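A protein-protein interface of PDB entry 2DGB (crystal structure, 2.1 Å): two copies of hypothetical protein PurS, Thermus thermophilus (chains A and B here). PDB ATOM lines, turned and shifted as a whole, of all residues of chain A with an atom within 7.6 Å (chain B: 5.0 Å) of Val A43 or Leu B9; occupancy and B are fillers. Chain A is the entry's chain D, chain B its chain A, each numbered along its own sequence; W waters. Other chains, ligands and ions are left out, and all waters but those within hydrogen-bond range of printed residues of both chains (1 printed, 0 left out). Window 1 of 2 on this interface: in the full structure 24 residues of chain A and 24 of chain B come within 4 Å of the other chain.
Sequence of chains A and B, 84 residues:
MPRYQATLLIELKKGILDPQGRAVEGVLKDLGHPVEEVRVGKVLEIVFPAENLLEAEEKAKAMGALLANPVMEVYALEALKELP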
ATOM      1  N   ALA A   6     -22.981  33.792  22.767  1.00  0.00           N
ATOM      2  CA  ALA A   6     -23.325  33.786  24.177  1.00  0.00           C
ATOM      3  C   ALA A   6     -24.140  32.539  24.484  1.00  0.00           C
ATOM      4  O   ALA A   6     -25.012  32.149  23.703  1.00  0.00           O
ATOM      5  CB  ALA A   6     -24.137  35.039  24.521  1.00  0.00           C
ATOM      6  N   THR A   7     -23.838  31.899  25.606  1.00  0.00           N
ATOM      7  CA  THR A   7     -24.586  30.722  26.028  1.00  0.00           C
ATOM      8  C   THR A   7     -25.360  31.159  27.262  1.00  0.00           C
ATOM      9  O   THR A   7     -24.768  31.397  28.318  1.00  0.00           O
ATOM     10  CB  THR A   7     -23.665  29.546  26.411  1.00  0.00           C
ATOM     11  OG1 THR A   7     -22.847  29.191  25.289  1.00  0.00           O
ATOM     12  CG2 THR A   7     -24.502  28.328  26.813  1.00  0.00           C
ATOM     13  N   LEU A   8     -26.677  31.281  27.125  1.00  0.00           N
ATOM     14  CA  LEU A   8     -27.517  31.710  28.239  1.00  0.00           C
ATOM     15  C   LEU A   8     -28.394  30.590  28.756  1.00  0.00           C
ATOM     16  O   LEU A   8     -28.984  29.836  27.975  1.00  0.00           O
ATOM     17  CB  LEU A   8     -28.411  32.871  27.818  1.00  0.00           C
ATOM     18  CG  LEU A   8     -27.764  34.214  27.502  1.00  0.00           C
ATOM     19  CD1 LEU A   8     -28.669  34.969  26.539  1.00  0.00           C
ATOM     20  CD2 LEU A   8     -27.539  35.013  28.787  1.00  0.00           C
ATOM     21  N   LEU A   9     -28.485  30.503  30.077  1.00  0.00           N
ATOM     22  CA  LEU A   9     -29.294  29.490  30.722  1.00  0.00           C
ATOM     23  C   LEU A   9     -30.464  30.163  31.423  1.00  0.00           C
ATOM     24  O   LEU A   9     -30.273  31.046  32.253  1.00  0.00           O
ATOM     25  CB  LEU A   9     -28.457  28.722  31.751  1.00  0.00           C
ATOM     26  CG  LEU A   9     -27.150  28.080  31.266  1.00  0.00           C
ATOM     27  CD1 LEU A   9     -26.487  27.365  32.437  1.00  0.00           C
ATOM     28  CD2 LEU A   9     -27.431  27.109  30.132  1.00  0.00           C
ATOM     29  N   ILE A  10     -31.678  29.760  31.069  1.00  0.00           N
ATOM     30  CA  ILE A  10     -32.870  30.306  31.701  1.00  0.00           C
ATOM     31  C   ILE A  10     -33.392  29.147  32.535  1.00  0.00           C
ATOM     32  O   ILE A  10     -33.886  28.160  31.989  1.00  0.00           O
ATOM     33  CB  ILE A  10     -33.934  30.714  30.664  1.00  0.00           C
ATOM     34  CG1 ILE A  10     -33.303  31.591  29.575  1.00  0.00           C
ATOM     35  CG2 ILE A  10     -35.068  31.464  31.355  1.00  0.00           C
ATOM     36  CD1 ILE A  10     -32.590  32.814  30.091  1.00  0.00           C
ATOM     37  N   GLU A  11     -33.256  29.252  33.855  1.00  0.00           N
ATOM     38  CA  GLU A  11     -33.695  28.177  34.733  1.00  0.00           C
ATOM     39  C   GLU A  11     -34.797  28.593  35.699  1.00  0.00           C
ATOM     40  O   GLU A  11     -35.008  29.779  35.951  1.00  0.00           O
ATOM     41  CB  GLU A  11     -32.488  27.607  35.498  1.00  0.00           C
ATOM     42  CG  GLU A  11     -31.292  27.342  34.599  1.00  0.00           C
ATOM     43  CD  GLU A  11     -30.270  26.394  35.207  1.00  0.00           C
ATOM     44  OE1 GLU A  11     -30.046  26.440  36.435  1.00  0.00           O
ATOM     45  OE2 GLU A  11     -29.678  25.602  34.447  1.00  0.00           O
ATOM     46  N   GLY A  41     -34.250  23.536  32.214  1.00  0.00           N
ATOM     47  CA  GLY A  41     -34.280  24.946  31.883  1.00  0.00           C
ATOM     48  C   GLY A  41     -34.052  25.082  30.390  1.00  0.00           C
ATOM     49  O   GLY A  41     -34.008  24.082  29.672  1.00  0.00           O
ATOM     50  N   LYS A  42     -33.917  26.316  29.918  1.00  0.00           N
ATOM     51  CA  LYS A  42     -33.676  26.572  28.509  1.00  0.00           C
ATOM     52  C   LYS A  42     -32.260  27.092  28.322  1.00  0.00           C
ATOM     53  O   LYS A  42     -31.753  27.842  29.152  1.00  0.00           O
ATOM     54  CB  LYS A  42     -34.669  27.617  27.976  1.00  0.00           C
ATOM     55  CG  LYS A  42     -36.104  27.134  27.896  1.00  0.00           C
ATOM     56  CD  LYS A  42     -37.092  28.282  27.710  1.00  0.00           C
ATOM     57  CE  LYS A  42     -37.355  29.011  29.018  1.00  0.00           C
ATOM     58  NZ  LYS A  42     -38.532  29.928  28.934  1.00  0.00           N
ATOM     59  N   VAL A  43     -31.609  26.672  27.245  1.00  0.00           N
ATOM     60  CA  VAL A  43     -30.274  27.168  26.945  1.00  0.00           C
ATOM     61  C   VAL A  43     -30.375  27.783  25.562  1.00  0.00           C
ATOM     62  O   VAL A  43     -30.923  27.168  24.647  1.00  0.00           O
ATOM     63  CB  VAL A  43     -29.207  26.044  26.931  1.00  0.00           C
ATOM     64  CG1 VAL A  43     -29.627  24.922  25.983  1.00  0.00           C
ATOM     65  CG2 VAL A  43     -27.861  26.620  26.490  1.00  0.00           C
ATOM     66  N   LEU A  44     -29.900  29.015  25.416  1.00  0.00           N
ATOM     67  CA  LEU A  44     -29.927  29.670  24.116  1.00  0.00           C
ATOM     68  C   LEU A  44     -28.526  30.047  23.663  1.00  0.00           C
ATOM     69  O   LEU A  44     -27.820  30.776  24.353  1.00  0.00           O
ATOM     70  CB  LEU A  44     -30.796  30.931  24.139  1.00  0.00           C
ATOM     71  CG  LEU A  44     -32.317  30.750  24.207  1.00  0.00           C
ATOM     72  CD1 LEU A  44     -32.768  30.718  25.661  1.00  0.00           C
ATOM     73  CD2 LEU A  44     -32.990  31.903  23.485  1.00  0.00           C
ATOM     74  N   GLU A  45     -28.124  29.526  22.507  1.00  0.00           N
ATOM     75  CA  GLU A  45     -26.825  29.839  21.930  1.00  0.00           C
ATOM     76  C   GLU A  45     -27.099  30.990  20.962  1.00  0.00           C
ATOM     77  O   GLU A  45     -27.715  30.792  19.911  1.00  0.00           O
ATOM     78  CB  GLU A  45     -26.269  28.636  21.159  1.00  0.00           C
ATOM     79  CG  GLU A  45     -26.119  27.346  21.970  1.00  0.00           C
ATOM     80  CD  GLU A  45     -25.060  27.435  23.057  1.00  0.00           C
ATOM     81  OE1 GLU A  45     -24.375  28.478  23.145  1.00  0.00           O
ATOM     82  OE2 GLU A  45     -24.910  26.453  23.822  1.00  0.00           O
ATOM     83  N   ILE A  46     -26.665  32.191  21.323  1.00  0.00           N
ATOM     84  CA  ILE A  46     -26.889  33.364  20.486  1.00  0.00           C
ATOM     85  C   ILE A  46     -25.607  33.932  19.886  1.00  0.00           C
ATOM     86  O   ILE A  46     -24.664  34.283  20.599  1.00  0.00           O
ATOM     87  CB  ILE A  46     -27.592  34.492  21.282  1.00  0.00           C
ATOM     88  CG1 ILE A  46     -28.895  33.960  21.890  1.00  0.00           C
ATOM     89  CG2 ILE A  46     -27.890  35.681  20.367  1.00  0.00           C
ATOM     90  CD1 ILE A  46     -29.696  35.008  22.640  1.00  0.00           C
ATOM     91  N   LEU A  67     -35.480  37.406  28.311  1.00  0.00           N
ATOM     92  CA  LEU A  67     -35.945  36.028  28.243  1.00  0.00           C
ATOM     93  C   LEU A  67     -36.529  35.404  29.507  1.00  0.00           C
ATOM     94  O   LEU A  67     -37.368  34.515  29.420  1.00  0.00           O
ATOM     95  CB  LEU A  67     -34.802  35.140  27.744  1.00  0.00           C
ATOM     96  CG  LEU A  67     -34.354  35.428  26.308  1.00  0.00           C
ATOM     97  CD1 LEU A  67     -32.948  34.885  26.072  1.00  0.00           C
ATOM     98  CD2 LEU A  67     -35.356  34.812  25.346  1.00  0.00           C
ATOM     99  N   GLU A  78     -23.803  31.728  30.933  1.00  0.00           N
ATOM    100  CA  GLU A  78     -22.932  30.577  31.164  1.00  0.00           C
ATOM    101  C   GLU A  78     -21.590  30.629  30.441  1.00  0.00           C
ATOM    102  O   GLU A  78     -20.583  30.122  30.942  1.00  0.00           O
ATOM    103  CB  GLU A  78     -23.692  29.303  30.777  1.00  0.00           C
ATOM    104  CG  GLU A  78     -22.857  28.041  30.643  1.00  0.00           C
ATOM    105  CD  GLU A  78     -22.166  27.655  31.924  1.00  0.00           C
ATOM    106  OE1 GLU A  78     -22.753  27.886  33.005  1.00  0.00           O
ATOM    107  OE2 GLU A  78     -21.042  27.105  31.850  1.00  0.00           O
ATOM    108  N   ALA A  79     -21.580  31.229  29.257  1.00  0.00           N
ATOM    109  CA  ALA A  79     -20.362  31.346  28.475  1.00  0.00           C
ATOM    110  C   ALA A  79     -20.492  32.469  27.454  1.00  0.00           C
ATOM    111  O   ALA A  79     -21.597  32.829  27.041  1.00  0.00           O
ATOM    112  CB  ALA A  79     -20.061  30.026  27.772  1.00  0.00           C
ATOM    113  N   THR B   7     -24.339  19.764  34.814  1.00  0.00           N
ATOM    114  CA  THR B   7     -25.054  20.721  33.980  1.00  0.00           C
ATOM    115  C   THR B   7     -24.913  20.198  32.552  1.00  0.00           C
ATOM    116  O   THR B   7     -23.858  20.341  31.923  1.00  0.00           O
ATOM    117  CB  THR B   7     -24.444  22.129  34.064  1.00  0.00           C
ATOM    118  OG1 THR B   7     -24.508  22.598  35.416  1.00  0.00           O
ATOM    119  CG2 THR B   7     -25.228  23.098  33.174  1.00  0.00           C
ATOM    120  N   LEU B   8     -25.975  19.572  32.058  1.00  0.00           N
ATOM    121  CA  LEU B   8     -25.986  18.999  30.718  1.00  0.00           C
ATOM    122  C   LEU B   8     -26.780  19.818  29.720  1.00  0.00           C
ATOM    123  O   LEU B   8     -27.952  20.129  29.942  1.00  0.00           O
ATOM    124  CB  LEU B   8     -26.571  17.585  30.748  1.00  0.00           C
ATOM    125  CG  LEU B   8     -25.683  16.407  31.148  1.00  0.00           C
ATOM    126  CD1 LEU B   8     -26.555  15.262  31.634  1.00  0.00           C
ATOM    127  CD2 LEU B   8     -24.833  15.970  29.964  1.00  0.00           C
ATOM    128  N   LEU B   9     -26.139  20.155  28.610  1.00  0.00           N
ATOM    129  CA  LEU B   9     -26.806  20.902  27.558  1.00  0.00           C
ATOM    130  C   LEU B   9     -27.179  19.893  26.473  1.00  0.00           C
ATOM    131  O   LEU B   9     -26.363  19.054  26.097  1.00  0.00           O
ATOM    132  CB  LEU B   9     -25.869  21.958  26.974  1.00  0.00           C
ATOM    133  CG  LEU B   9     -25.303  23.001  27.937  1.00  0.00           C
ATOM    134  CD1 LEU B   9     -24.447  23.982  27.153  1.00  0.00           C
ATOM    135  CD2 LEU B   9     -26.441  23.732  28.647  1.00  0.00           C
ATOM    136  N   ILE B  10     -28.418  19.957  25.995  1.00  0.00           N
ATOM    137  CA  ILE B  10     -28.865  19.065  24.932  1.00  0.00           C
ATOM    138  C   ILE B  10     -29.386  19.977  23.834  1.00  0.00           C
ATOM    139  O   ILE B  10     -30.426  20.627  23.975  1.00  0.00           O
ATOM    140  CB  ILE B  10     -29.965  18.094  25.434  1.00  0.00           C
ATOM    141  CG1 ILE B  10     -29.377  17.175  26.521  1.00  0.00           C
ATOM    142  CG2 ILE B  10     -30.489  17.261  24.281  1.00  0.00           C
ATOM    143  CD1 ILE B  10     -30.376  16.200  27.140  1.00  0.00           C
ATOM    144  N   GLU B  11     -28.638  20.047  22.742  1.00  0.00           N
ATOM    145  CA  GLU B  11     -29.012  20.929  21.656  1.00  0.00           C
ATOM    146  C   GLU B  11     -29.134  20.176  20.338  1.00  0.00           C
ATOM    147  O   GLU B  11     -28.653  19.051  20.200  1.00  0.00           O
ATOM    148  CB  GLU B  11     -27.971  22.048  21.540  1.00  0.00           C
ATOM    149  CG  GLU B  11     -27.506  22.583  22.901  1.00  0.00           C
ATOM    150  CD  GLU B  11     -26.537  23.754  22.795  1.00  0.00           C
ATOM    151  OE1 GLU B  11     -25.712  23.776  21.861  1.00  0.00           O
ATOM    152  OE2 GLU B  11     -26.594  24.650  23.662  1.00  0.00           O
ATOM    153  N   ARG B  39     -30.071  29.503  18.654  1.00  0.00           N
ATOM    154  CA  ARG B  39     -30.348  28.066  18.672  1.00  0.00           C
ATOM    155  C   ARG B  39     -30.880  27.808  20.071  1.00  0.00           C
ATOM    156  O   ARG B  39     -30.220  28.140  21.058  1.00  0.00           O
ATOM    157  CB  ARG B  39     -29.081  27.241  18.431  1.00  0.00           C
ATOM    158  CG  ARG B  39     -28.478  27.399  17.048  1.00  0.00           C
ATOM    159  CD  ARG B  39     -29.408  26.871  15.957  1.00  0.00           C
ATOM    160  NE  ARG B  39     -29.426  25.408  15.888  1.00  0.00           N
ATOM    161  CZ  ARG B  39     -30.018  24.716  14.917  1.00  0.00           C
ATOM    162  NH1 ARG B  39     -30.646  25.355  13.934  1.00  0.00           N
ATOM    163  NH2 ARG B  39     -29.967  23.387  14.907  1.00  0.00           N
ATOM    164  N   VAL B  40     -32.079  27.243  20.156  1.00  0.00           N
ATOM    165  CA  VAL B  40     -32.708  26.983  21.444  1.00  0.00           C
ATOM    166  C   VAL B  40     -32.606  25.521  21.827  1.00  0.00           C
ATOM    167  O   VAL B  40     -33.008  24.632  21.068  1.00  0.00           O
ATOM    168  CB  VAL B  40     -34.201  27.401  21.435  1.00  0.00           C
ATOM    169  CG1 VAL B  40     -34.848  27.076  22.773  1.00  0.00           C
ATOM    170  CG2 VAL B  40     -34.318  28.892  21.151  1.00  0.00           C
ATOM    171  N   GLY B  41     -32.049  25.282  23.007  1.00  0.00           N
ATOM    172  CA  GLY B  41     -31.896  23.930  23.491  1.00  0.00           C
ATOM    173  C   GLY B  41     -32.419  23.832  24.907  1.00  0.00           C
ATOM    174  O   GLY B  41     -33.099  24.734  25.403  1.00  0.00           O
ATOM    175  N   LYS B  42     -32.104  22.728  25.565  1.00  0.00           N
ATOM    176  CA  LYS B  42     -32.545  22.534  26.931  1.00  0.00           C
ATOM    177  C   LYS B  42     -31.333  22.315  27.825  1.00  0.00           C
ATOM    178  O   LYS B  42     -30.319  21.766  27.392  1.00  0.00           O
ATOM    179  CB  LYS B  42     -33.476  21.317  27.010  1.00  0.00           C
ATOM    180  CG  LYS B  42     -32.756  19.990  26.903  1.00  0.00           C
ATOM    181  CD  LYS B  42     -33.720  18.820  26.687  1.00  0.00           C
ATOM    182  CE  LYS B  42     -34.252  18.779  25.255  1.00  0.00           C
ATOM    183  NZ  LYS B  42     -34.924  17.482  24.940  1.00  0.00           N
ATOM    184  N   VAL B  43     -31.424  22.786  29.060  1.00  0.00           N
ATOM    185  CA  VAL B  43     -30.348  22.576  30.016  1.00  0.00           C
ATOM    186  C   VAL B  43     -30.944  21.749  31.147  1.00  0.00           C
ATOM    187  O   VAL B  43     -32.063  22.022  31.609  1.00  0.00           O
ATOM    188  CB  VAL B  43     -29.768  23.913  30.585  1.00  0.00           C
ATOM    189  CG1 VAL B  43     -30.859  24.737  31.261  1.00  0.00           C
ATOM    190  CG2 VAL B  43     -28.644  23.604  31.589  1.00  0.00           C
ATOM    191  N   VAL B  74     -27.123  16.640  20.172  1.00  0.00           N
ATOM    192  CA  VAL B  74     -25.797  16.392  20.710  1.00  0.00           C
ATOM    193  C   VAL B  74     -25.869  16.895  22.146  1.00  0.00           C
ATOM    194  O   VAL B  74     -26.601  17.846  22.438  1.00  0.00           O
ATOM    195  CB  VAL B  74     -24.706  17.184  19.957  1.00  0.00           C
ATOM    196  CG1 VAL B  74     -24.575  16.669  18.525  1.00  0.00           C
ATOM    197  CG2 VAL B  74     -25.041  18.663  19.964  1.00  0.00           C
ATOM    198  N   TYR B  75     -25.141  16.251  23.047  1.00  0.00           N
ATOM    199  CA  TYR B  75     -25.147  16.693  24.434  1.00  0.00           C
ATOM    200  C   TYR B  75     -23.758  17.175  24.782  1.00  0.00           C
ATOM    201  O   TYR B  75     -22.782  16.824  24.118  1.00  0.00           O
ATOM    202  CB  TYR B  75     -25.557  15.550  25.375  1.00  0.00           C
ATOM    203  CG  TYR B  75     -24.591  14.382  25.413  1.00  0.00           C
ATOM    204  CD1 TYR B  75     -23.505  14.365  26.293  1.00  0.00           C
ATOM    205  CD2 TYR B  75     -24.765  13.290  24.567  1.00  0.00           C
ATOM    206  CE1 TYR B  75     -22.617  13.280  26.327  1.00  0.00           C
ATOM    207  CE2 TYR B  75     -23.888  12.207  24.591  1.00  0.00           C
ATOM    208  CZ  TYR B  75     -22.822  12.203  25.469  1.00  0.00           C
ATOM    209  OH  TYR B  75     -21.983  11.105  25.491  1.00  0.00           O
ATOM    210  N   ALA B  76     -23.672  17.989  25.823  1.00  0.00           N
ATOM    211  CA  ALA B  76     -22.392  18.506  26.269  1.00  0.00           C
ATOM    212  C   ALA B  76     -22.434  18.680  27.779  1.00  0.00           C
ATOM    213  O   ALA B  76     -23.364  19.296  28.309  1.00  0.00           O
ATOM    214  CB  ALA B  76     -22.106  19.842  25.594  1.00  0.00           C
ATOM    215  N   GLU B  78     -21.560  20.629  30.393  1.00  0.00           N
ATOM    216  CA  GLU B  78     -21.091  21.992  30.603  1.00  0.00           C
ATOM    217  C   GLU B  78     -20.347  22.200  31.925  1.00  0.00           C
ATOM    218  O   GLU B  78     -19.416  23.002  31.997  1.00  0.00           O
ATOM    219  CB  GLU B  78     -22.276  22.950  30.516  1.00  0.00           C
ATOM    220  CG  GLU B  78     -21.923  24.422  30.611  1.00  0.00           C
ATOM    221  CD  GLU B  78     -21.037  24.890  29.471  1.00  0.00           C
ATOM    222  OE1 GLU B  78     -21.110  24.289  28.375  1.00  0.00           O
ATOM    223  OE2 GLU B  78     -20.282  25.868  29.667  1.00  0.00           O
HETATM  224  O   HOH W   1     -21.085  26.890  26.536  1.00  0.00           O
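Water W1 lies within hydrogen-bond range of the side-chain hydroxyl of Thr A7 and the side-chain carboxylate of Glu B78.
Leu B9 touches two residues of chain A. Of chain A, only Lys A42 (3.7 Å) and Val A43 (2.7 Å) come within 4 Å of Gly B41. Printed residues of chain A within 4 Å of Glu B78: Glu A78 (2.6 Å). Printed residues of chain B within 4 Å of Gly A41: Lys B42 (3.5 Å) and Val B43 (2.7 Å). Ile B10 touches none of the printed residues of chain A. The nearest residue of chain B that does not touch Val A43 is Val B43 (4.2 Å). The nearest residue of chain A that does not touch Leu B9 is Glu A45 (4.2 Å). The nearest printed residue of chain A that does not touch Glu B78 is Ala A79 (4.6 Å).
Leu B9 touches Leu A9 (CD2 to CD2, 3.8 Å). Val B43 touches Leu A9. Glu A11 touches Val B43. O of Gly A41 touches CA of Lys B42, at 3.5 Å. Val B43 touches Lys A42. Val A43 touches Leu B9 (CG2 to CD2, 3.9 Å). CG2 of Val A43 touches OE2 of Glu B11, 3.7 Å away. Arg B39 touches Val A43. Val A43 touches Val B40 (O to CA, 3.7 Å). Lys B42 touches Val A43.
Of the 14 printed residues of chain B, 8 touch a printed residue of chain A. Printed residues of chain B that touch a printed residue of chain A: Leu B9, Glu B11, Arg B39, Val B40, Gly B41, Lys B42, Val B43 and Glu B78. Among the printed residues, no Asp or Glu carboxylate lies within 4 Å of a Lys or Arg side-chain nitrogen of the other chain.
OE2 of Glu B78 sits close to OE2 of Glu A78. N of Gly A41 sits at hydrogen-bond distance from O of Val B43. The side-chain carboxylate (OE2) of Glu A45 lies close to the side-chain carboxylate (OE2) of Glu B11, 2.5 Å away. The backbone NH of Glu A45 lies within hydrogen-bond range of the backbone carbonyl oxygen of Arg B39 (2.9 Å). The backbone carbonyl oxygen of Val A43 lies within hydrogen-bond range of the backbone NH of Gly B41, 2.7 Å away.
The side-chain carboxylate of Glu A45 is in hydrogen-bond range of the side-chain hydroxyl of Thr A7 (2.7 Å). O of Thr A7 is in hydrogen-bond range of N of Glu A78 (2.8 Å). The backbone NH (N) of Leu A44 sits at hydrogen-bond distance from the backbone carbonyl oxygen (O) of Leu A8. The backbone NH (N) of Glu B78 is in hydrogen-bond range of the backbone carbonyl oxygen (O) of Thr B7, 2.8 Å away. The backbone carbonyl oxygen (O) of Glu B11 lies within hydrogen-bond range of the backbone NH (N) of Val B74 (2.9 Å). The backbone carbonyl oxygen (O) of Lys B42 lies within hydrogen-bond range of the backbone NH (N) of Ile B10 (3.0 Å).
Leu B9 touches its own counterpart, Leu A9. Glu A11 touches Val B43, and with the chains exchanged Val A43 touches Glu B11. Gly A41 touches Val B43, and with the chains exchanged Val A43 touches Gly B41. Lys A42 touches Val B43, and with the chains exchanged Val A43 touches Lys B42. Of the 17 pairs that touch across the chains among the printed residues, 12 have their exchanged pair printed and touching as well.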
